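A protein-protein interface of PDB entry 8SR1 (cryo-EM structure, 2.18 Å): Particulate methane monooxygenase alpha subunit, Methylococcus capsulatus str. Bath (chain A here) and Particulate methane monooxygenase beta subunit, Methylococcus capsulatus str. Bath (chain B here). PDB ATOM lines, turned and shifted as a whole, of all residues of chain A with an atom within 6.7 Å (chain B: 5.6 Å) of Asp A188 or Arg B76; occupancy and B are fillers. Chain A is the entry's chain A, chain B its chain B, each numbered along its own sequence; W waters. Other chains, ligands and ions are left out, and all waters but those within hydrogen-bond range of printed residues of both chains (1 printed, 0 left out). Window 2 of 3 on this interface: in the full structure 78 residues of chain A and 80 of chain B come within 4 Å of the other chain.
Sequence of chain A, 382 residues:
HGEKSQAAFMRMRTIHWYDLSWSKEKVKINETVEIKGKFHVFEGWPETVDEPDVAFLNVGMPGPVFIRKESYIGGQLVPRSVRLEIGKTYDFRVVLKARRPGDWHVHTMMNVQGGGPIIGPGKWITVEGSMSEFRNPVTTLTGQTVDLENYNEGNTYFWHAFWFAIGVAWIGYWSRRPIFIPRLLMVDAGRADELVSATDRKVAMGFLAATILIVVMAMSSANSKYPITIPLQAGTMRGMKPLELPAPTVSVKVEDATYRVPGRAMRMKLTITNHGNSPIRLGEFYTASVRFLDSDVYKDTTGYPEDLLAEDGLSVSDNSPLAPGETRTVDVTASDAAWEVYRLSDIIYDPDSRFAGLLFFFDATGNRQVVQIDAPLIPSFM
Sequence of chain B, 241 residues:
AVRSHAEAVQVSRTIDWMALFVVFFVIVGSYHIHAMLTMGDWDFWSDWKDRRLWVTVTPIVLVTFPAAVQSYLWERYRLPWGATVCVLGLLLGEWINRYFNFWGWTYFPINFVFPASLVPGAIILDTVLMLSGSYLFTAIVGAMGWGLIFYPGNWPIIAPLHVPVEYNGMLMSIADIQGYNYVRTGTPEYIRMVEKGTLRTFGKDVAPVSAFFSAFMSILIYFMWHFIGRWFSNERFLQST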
ATOM      1  N   PHE A 180     -10.971 -18.434   3.324  1.00  0.00           N
ATOM      2  CA  PHE A 180     -10.095 -19.135   2.389  1.00  0.00           C
ATOM      3  C   PHE A 180     -10.677 -20.432   1.836  1.00  0.00           C
ATOM      4  O   PHE A 180     -10.904 -20.542   0.629  1.00  0.00           O
ATOM      5  CB  PHE A 180      -8.746 -19.413   3.064  1.00  0.00           C
ATOM      6  CG  PHE A 180      -7.858 -18.209   3.146  1.00  0.00           C
ATOM      7  CD1 PHE A 180      -7.369 -17.616   1.995  1.00  0.00           C
ATOM      8  CD2 PHE A 180      -7.513 -17.667   4.371  1.00  0.00           C
ATOM      9  CE1 PHE A 180      -6.553 -16.507   2.066  1.00  0.00           C
ATOM     10  CE2 PHE A 180      -6.697 -16.557   4.447  1.00  0.00           C
ATOM     11  CZ  PHE A 180      -6.216 -15.975   3.292  1.00  0.00           C
ATOM     12  N   ARG A 183     -14.471 -20.510   0.368  1.00  0.00           N
ATOM     13  CA  ARG A 183     -14.508 -19.716  -0.858  1.00  0.00           C
ATOM     14  C   ARG A 183     -13.750 -20.409  -1.982  1.00  0.00           C
ATOM     15  O   ARG A 183     -14.189 -20.394  -3.138  1.00  0.00           O
ATOM     16  CB  ARG A 183     -13.945 -18.316  -0.608  1.00  0.00           C
ATOM     17  CG  ARG A 183     -14.859 -17.420   0.210  1.00  0.00           C
ATOM     18  CD  ARG A 183     -14.302 -16.017   0.347  1.00  0.00           C
ATOM     19  NE  ARG A 183     -14.655 -15.170  -0.785  1.00  0.00           N
ATOM     20  CZ  ARG A 183     -15.721 -14.383  -0.827  1.00  0.00           C
ATOM     21  NH1 ARG A 183     -16.575 -14.323   0.179  1.00  0.00           N
ATOM     22  NH2 ARG A 183     -15.934 -13.637  -1.908  1.00  0.00           N
ATOM     23  N   LEU A 184     -12.608 -21.024  -1.662  1.00  0.00           N
ATOM     24  CA  LEU A 184     -11.864 -21.783  -2.661  1.00  0.00           C
ATOM     25  C   LEU A 184     -12.699 -22.936  -3.203  1.00  0.00           C
ATOM     26  O   LEU A 184     -12.733 -23.173  -4.417  1.00  0.00           O
ATOM     27  CB  LEU A 184     -10.566 -22.306  -2.051  1.00  0.00           C
ATOM     28  CG  LEU A 184      -9.744 -23.309  -2.858  1.00  0.00           C
ATOM     29  CD1 LEU A 184      -9.094 -22.627  -4.047  1.00  0.00           C
ATOM     30  CD2 LEU A 184      -8.700 -23.976  -1.979  1.00  0.00           C
ATOM     31  N   LEU A 185     -13.382 -23.661  -2.314  1.00  0.00           N
ATOM     32  CA  LEU A 185     -14.222 -24.771  -2.748  1.00  0.00           C
ATOM     33  C   LEU A 185     -15.390 -24.286  -3.598  1.00  0.00           C
ATOM     34  O   LEU A 185     -15.755 -24.931  -4.583  1.00  0.00           O
ATOM     35  CB  LEU A 185     -14.728 -25.552  -1.537  1.00  0.00           C
ATOM     36  CG  LEU A 185     -13.685 -26.378  -0.781  1.00  0.00           C
ATOM     37  CD1 LEU A 185     -14.281 -26.955   0.491  1.00  0.00           C
ATOM     38  CD2 LEU A 185     -13.126 -27.476  -1.663  1.00  0.00           C
ATOM     39  N   MET A 186     -15.994 -23.157  -3.223  1.00  0.00           N
ATOM     40  CA  MET A 186     -17.092 -22.612  -4.015  1.00  0.00           C
ATOM     41  C   MET A 186     -16.620 -22.198  -5.405  1.00  0.00           C
ATOM     42  O   MET A 186     -17.318 -22.438  -6.396  1.00  0.00           O
ATOM     43  CB  MET A 186     -17.723 -21.424  -3.290  1.00  0.00           C
ATOM     44  CG  MET A 186     -18.602 -21.816  -2.116  1.00  0.00           C
ATOM     45  SD  MET A 186     -20.215 -22.416  -2.642  1.00  0.00           S
ATOM     46  CE  MET A 186     -20.914 -20.925  -3.341  1.00  0.00           C
ATOM     47  N   VAL A 187     -15.447 -21.569  -5.492  1.00  0.00           N
ATOM     48  CA  VAL A 187     -14.932 -21.155  -6.795  1.00  0.00           C
ATOM     49  C   VAL A 187     -14.586 -22.368  -7.648  1.00  0.00           C
ATOM     50  O   VAL A 187     -14.877 -22.401  -8.851  1.00  0.00           O
ATOM     51  CB  VAL A 187     -13.724 -20.218  -6.620  1.00  0.00           C
ATOM     52  CG1 VAL A 187     -13.049 -19.967  -7.955  1.00  0.00           C
ATOM     53  CG2 VAL A 187     -14.158 -18.902  -5.994  1.00  0.00           C
ATOM     54  N   ASP A 188     -13.967 -23.388  -7.049  1.00  0.00           N
ATOM     55  CA  ASP A 188     -13.557 -24.568  -7.811  1.00  0.00           C
ATOM     56  C   ASP A 188     -14.762 -25.385  -8.267  1.00  0.00           C
ATOM     57  O   ASP A 188     -14.959 -25.613  -9.465  1.00  0.00           O
ATOM     58  CB  ASP A 188     -12.606 -25.430  -6.973  1.00  0.00           C
ATOM     59  CG  ASP A 188     -11.236 -24.801  -6.817  1.00  0.00           C
ATOM     60  OD1 ASP A 188     -10.754 -24.170  -7.780  1.00  0.00           O
ATOM     61  OD2 ASP A 188     -10.638 -24.944  -5.731  1.00  0.00           O
ATOM     62  N   ALA A 189     -15.582 -25.834  -7.318  1.00  0.00           N
ATOM     63  CA  ALA A 189     -16.724 -26.682  -7.639  1.00  0.00           C
ATOM     64  C   ALA A 189     -17.849 -25.859  -8.248  1.00  0.00           C
ATOM     65  O   ALA A 189     -18.682 -25.299  -7.529  1.00  0.00           O
ATOM     66  CB  ALA A 189     -17.214 -27.417  -6.391  1.00  0.00           C
ATOM     67  N   GLY A 190     -17.881 -25.786  -9.575  1.00  0.00           N
ATOM     68  CA  GLY A 190     -18.892 -25.023 -10.270  1.00  0.00           C
ATOM     69  C   GLY A 190     -18.588 -23.539 -10.281  1.00  0.00           C
ATOM     70  O   GLY A 190     -17.611 -23.057  -9.708  1.00  0.00           O
ATOM     71  N   ARG A 191     -19.459 -22.799 -10.962  1.00  0.00           N
ATOM     72  CA  ARG A 191     -19.345 -21.351 -10.989  1.00  0.00           C
ATOM     73  C   ARG A 191     -19.631 -20.788  -9.602  1.00  0.00           C
ATOM     74  O   ARG A 191     -20.512 -21.265  -8.882  1.00  0.00           O
ATOM     75  CB  ARG A 191     -20.319 -20.764 -12.010  1.00  0.00           C
ATOM     76  CG  ARG A 191     -19.871 -20.911 -13.451  1.00  0.00           C
ATOM     77  CD  ARG A 191     -20.963 -20.452 -14.401  1.00  0.00           C
ATOM     78  NE  ARG A 191     -20.545 -20.535 -15.796  1.00  0.00           N
ATOM     79  CZ  ARG A 191     -21.345 -20.883 -16.794  1.00  0.00           C
ATOM     80  NH1 ARG A 191     -22.617 -21.180 -16.587  1.00  0.00           N
ATOM     81  NH2 ARG A 191     -20.854 -20.940 -18.029  1.00  0.00           N
ATOM     82  N   ALA A 192     -18.872 -19.763  -9.217  1.00  0.00           N
ATOM     83  CA  ALA A 192     -19.059 -19.249  -7.869  1.00  0.00           C
ATOM     84  C   ALA A 192     -20.238 -18.290  -7.812  1.00  0.00           C
ATOM     85  O   ALA A 192     -21.295 -18.642  -7.279  1.00  0.00           O
ATOM     86  CB  ALA A 192     -17.788 -18.547  -7.389  1.00  0.00           C
ATOM     87  N   SER B  71      -4.219 -11.344  -8.847  1.00  0.00           N
ATOM     88  CA  SER B  71      -4.422 -12.414  -9.816  1.00  0.00           C
ATOM     89  C   SER B  71      -4.597 -13.762  -9.137  1.00  0.00           C
ATOM     90  O   SER B  71      -5.204 -14.672  -9.707  1.00  0.00           O
ATOM     91  CB  SER B  71      -3.246 -12.470 -10.790  1.00  0.00           C
ATOM     92  OG  SER B  71      -2.228 -13.332 -10.310  1.00  0.00           O
ATOM     93  N   TYR B  72      -4.059 -13.913  -7.929  1.00  0.00           N
ATOM     94  CA  TYR B  72      -4.276 -15.160  -7.199  1.00  0.00           C
ATOM     95  C   TYR B  72      -5.560 -15.114  -6.374  1.00  0.00           C
ATOM     96  O   TYR B  72      -6.430 -15.982  -6.512  1.00  0.00           O
ATOM     97  CB  TYR B  72      -3.077 -15.457  -6.305  1.00  0.00           C
ATOM     98  CG  TYR B  72      -3.311 -16.558  -5.297  1.00  0.00           C
ATOM     99  CD1 TYR B  72      -3.397 -17.884  -5.695  1.00  0.00           C
ATOM    100  CD2 TYR B  72      -3.435 -16.271  -3.944  1.00  0.00           C
ATOM    101  CE1 TYR B  72      -3.604 -18.890  -4.776  1.00  0.00           C
ATOM    102  CE2 TYR B  72      -3.641 -17.271  -3.017  1.00  0.00           C
ATOM    103  CZ  TYR B  72      -3.725 -18.581  -3.439  1.00  0.00           C
ATOM    104  OH  TYR B  72      -3.933 -19.581  -2.522  1.00  0.00           O
ATOM    105  N   LEU B  73      -5.683 -14.114  -5.499  1.00  0.00           N
ATOM    106  CA  LEU B  73      -6.777 -14.087  -4.537  1.00  0.00           C
ATOM    107  C   LEU B  73      -8.125 -13.952  -5.228  1.00  0.00           C
ATOM    108  O   LEU B  73      -9.054 -14.710  -4.939  1.00  0.00           O
ATOM    109  CB  LEU B  73      -6.571 -12.945  -3.539  1.00  0.00           C
ATOM    110  CG  LEU B  73      -5.531 -13.177  -2.443  1.00  0.00           C
ATOM    111  CD1 LEU B  73      -5.535 -12.024  -1.456  1.00  0.00           C
ATOM    112  CD2 LEU B  73      -5.785 -14.496  -1.728  1.00  0.00           C
ATOM    113  N   TRP B  74      -8.259 -12.990  -6.145  1.00  0.00           N
ATOM    114  CA  TRP B  74      -9.536 -12.824  -6.829  1.00  0.00           C
ATOM    115  C   TRP B  74      -9.893 -14.072  -7.621  1.00  0.00           C
ATOM    116  O   TRP B  74     -11.005 -14.598  -7.504  1.00  0.00           O
ATOM    117  CB  TRP B  74      -9.494 -11.596  -7.736  1.00  0.00           C
ATOM    118  CG  TRP B  74     -10.759 -11.391  -8.500  1.00  0.00           C
ATOM    119  CD1 TRP B  74     -10.940 -11.549  -9.841  1.00  0.00           C
ATOM    120  CD2 TRP B  74     -12.032 -11.017  -7.963  1.00  0.00           C
ATOM    121  NE1 TRP B  74     -12.244 -11.281 -10.178  1.00  0.00           N
ATOM    122  CE2 TRP B  74     -12.935 -10.952  -9.041  1.00  0.00           C
ATOM    123  CE3 TRP B  74     -12.494 -10.723  -6.677  1.00  0.00           C
ATOM    124  CZ2 TRP B  74     -14.273 -10.607  -8.873  1.00  0.00           C
ATOM    125  CZ3 TRP B  74     -13.820 -10.382  -6.513  1.00  0.00           C
ATOM    126  CH2 TRP B  74     -14.696 -10.328  -7.605  1.00  0.00           C
ATOM    127  N   GLU B  75      -8.933 -14.600  -8.384  1.00  0.00           N
ATOM    128  CA  GLU B  75      -9.212 -15.749  -9.239  1.00  0.00           C
ATOM    129  C   GLU B  75      -9.609 -16.981  -8.434  1.00  0.00           C
ATOM    130  O   GLU B  75     -10.494 -17.732  -8.856  1.00  0.00           O
ATOM    131  CB  GLU B  75      -7.998 -16.060 -10.112  1.00  0.00           C
ATOM    132  CG  GLU B  75      -8.248 -17.082 -11.217  1.00  0.00           C
ATOM    133  CD  GLU B  75      -9.244 -16.608 -12.264  1.00  0.00           C
ATOM    134  OE1 GLU B  75      -9.556 -15.399 -12.305  1.00  0.00           O
ATOM    135  OE2 GLU B  75      -9.713 -17.454 -13.053  1.00  0.00           O
ATOM    136  N   ARG B  76      -8.978 -17.211  -7.282  1.00  0.00           N
ATOM    137  CA  ARG B  76      -9.193 -18.461  -6.567  1.00  0.00           C
ATOM    138  C   ARG B  76     -10.219 -18.372  -5.444  1.00  0.00           C
ATOM    139  O   ARG B  76     -10.774 -19.408  -5.062  1.00  0.00           O
ATOM    140  CB  ARG B  76      -7.867 -18.977  -5.993  1.00  0.00           C
ATOM    141  CG  ARG B  76      -6.846 -19.367  -7.050  1.00  0.00           C
ATOM    142  CD  ARG B  76      -7.470 -20.200  -8.162  1.00  0.00           C
ATOM    143  NE  ARG B  76      -8.035 -21.450  -7.665  1.00  0.00           N
ATOM    144  CZ  ARG B  76      -7.353 -22.576  -7.527  1.00  0.00           C
ATOM    145  NH1 ARG B  76      -6.072 -22.652  -7.845  1.00  0.00           N
ATOM    146  NH2 ARG B  76      -7.972 -23.658  -7.062  1.00  0.00           N
ATOM    147  N   TYR B  77     -10.496 -17.183  -4.904  1.00  0.00           N
ATOM    148  CA  TYR B  77     -11.411 -17.066  -3.779  1.00  0.00           C
ATOM    149  C   TYR B  77     -12.431 -15.947  -3.935  1.00  0.00           C
ATOM    150  O   TYR B  77     -13.296 -15.815  -3.065  1.00  0.00           O
ATOM    151  CB  TYR B  77     -10.630 -16.832  -2.471  1.00  0.00           C
ATOM    152  CG  TYR B  77      -9.423 -17.718  -2.268  1.00  0.00           C
ATOM    153  CD1 TYR B  77      -8.196 -17.400  -2.836  1.00  0.00           C
ATOM    154  CD2 TYR B  77      -9.501 -18.864  -1.491  1.00  0.00           C
ATOM    155  CE1 TYR B  77      -7.090 -18.203  -2.646  1.00  0.00           C
ATOM    156  CE2 TYR B  77      -8.403 -19.669  -1.293  1.00  0.00           C
ATOM    157  CZ  TYR B  77      -7.201 -19.337  -1.873  1.00  0.00           C
ATOM    158  OH  TYR B  77      -6.103 -20.140  -1.680  1.00  0.00           O
ATOM    159  N   ARG B  78     -12.363 -15.145  -4.999  1.00  0.00           N
ATOM    160  CA  ARG B  78     -13.174 -13.936  -5.134  1.00  0.00           C
ATOM    161  C   ARG B  78     -12.990 -13.019  -3.928  1.00  0.00           C
ATOM    162  O   ARG B  78     -13.943 -12.434  -3.409  1.00  0.00           O
ATOM    163  CB  ARG B  78     -14.648 -14.274  -5.351  1.00  0.00           C
ATOM    164  CG  ARG B  78     -14.923 -14.947  -6.681  1.00  0.00           C
ATOM    165  CD  ARG B  78     -14.868 -13.941  -7.819  1.00  0.00           C
ATOM    166  NE  ARG B  78     -15.004 -14.567  -9.128  1.00  0.00           N
ATOM    167  CZ  ARG B  78     -14.084 -15.334  -9.698  1.00  0.00           C
ATOM    168  NH1 ARG B  78     -12.921 -15.574  -9.111  1.00  0.00           N
ATOM    169  NH2 ARG B  78     -14.331 -15.865 -10.891  1.00  0.00           N
ATOM    170  N   GLU B 235       0.334 -25.213  -8.824  1.00  0.00           N
ATOM    171  CA  GLU B 235       0.269 -26.269  -7.820  1.00  0.00           C
ATOM    172  C   GLU B 235       0.946 -27.535  -8.323  1.00  0.00           C
ATOM    173  O   GLU B 235       0.548 -28.652  -7.980  1.00  0.00           O
ATOM    174  CB  GLU B 235      -1.177 -26.561  -7.430  1.00  0.00           C
ATOM    175  CG  GLU B 235      -1.948 -25.351  -6.939  1.00  0.00           C
ATOM    176  CD  GLU B 235      -3.371 -25.321  -7.458  1.00  0.00           C
ATOM    177  OE1 GLU B 235      -4.015 -26.391  -7.499  1.00  0.00           O
ATOM    178  OE2 GLU B 235      -3.846 -24.228  -7.831  1.00  0.00           O
HETATM  179  O   HOH W   1     -10.725 -21.787  -6.838  1.00  0.00           O
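The guanidinium group of Arg A183 is in hydrogen-bond range of the backbone carbonyl oxygen of Tyr B77, at 2.7 Å. O of Arg B78 lies within hydrogen-bond range of NH2 of Arg A183 (2.8 Å). OD1 of Asp A188 lies within salt-bridge range of NH2 of Arg B76 (2.9 Å).
Hydrophobic or aromatic side chains of chain B that line the printed part of chain A: Tyr B77. Of the 11 printed residues of chain A, 5 touch a printed residue of chain B. Hydrophobic or aromatic side chains of chain A that line the printed part of chain B: Leu A184 and Val A187. Among the printed residues, 9 pairs touch across the chains. Among the printed residues, Asp or Glu carboxylates within 4 Å of a Lys or Arg side-chain nitrogen of the other chain: Asp A188 with Arg B76.
The backbone NH (N) of Arg B78 lies within hydrogen-bond range of the backbone carbonyl oxygen (O) of Leu B73 (3.3 Å). The backbone carbonyl oxygen of Trp B74 lies within hydrogen-bond range of the guanidinium group of Arg B78 (2.7 Å). The backbone carbonyl oxygen of Glu B75 lies within hydrogen-bond range of the guanidinium group of Arg B78 (3.3 Å). The guanidinium group of Arg B76 lies within salt-bridge range of the side-chain carboxylate of Glu B235, at 2.7 Å.
Printed residues of chain B within 4 Å of Asp A188: Arg B76. Of chain A, only Leu A184, Val A187 and Asp A188 come within 4 Å of Arg B76. Printed residues of chain B within 4 Å of Phe A180: Tyr B77 (3.0 Å). Printed residues of chain B within 4 Å of Val A187: Glu B75 (3.5 Å), Arg B76 (3.4 Å) and Tyr B77 (3.98 Å). Of the printed residues of chain A, Arg B78 touches Arg A183. The nearest printed residue of chain B that does not touch Asp A188 is Glu B75 (6.5 Å). The nearest residue of chain A that does not touch Arg B76 is Arg A183 (4.04 Å). The nearest printed residue of chain B that does not touch Arg A183 is Arg B76 (4.04 Å).
Water W1 lies within hydrogen-bond range of the side-chain carboxylate (OD1) of Asp A188, the guanidinium group (NE) of Arg B76 and the backbone carbonyl oxygen (O) of Leu A184.
Among the printed residues, merely in contact across the chains: Phe A180 with Tyr B77 (3.0 Å), Leu A184 with Arg B76 (3.4 Å), Leu A184 with Tyr B77 (3.5 Å), Val A187 with Glu B75 (3.5 Å), Val A187 with Arg B76 (3.4 Å) and Val A187 with Tyr B77 (3.98 Å).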
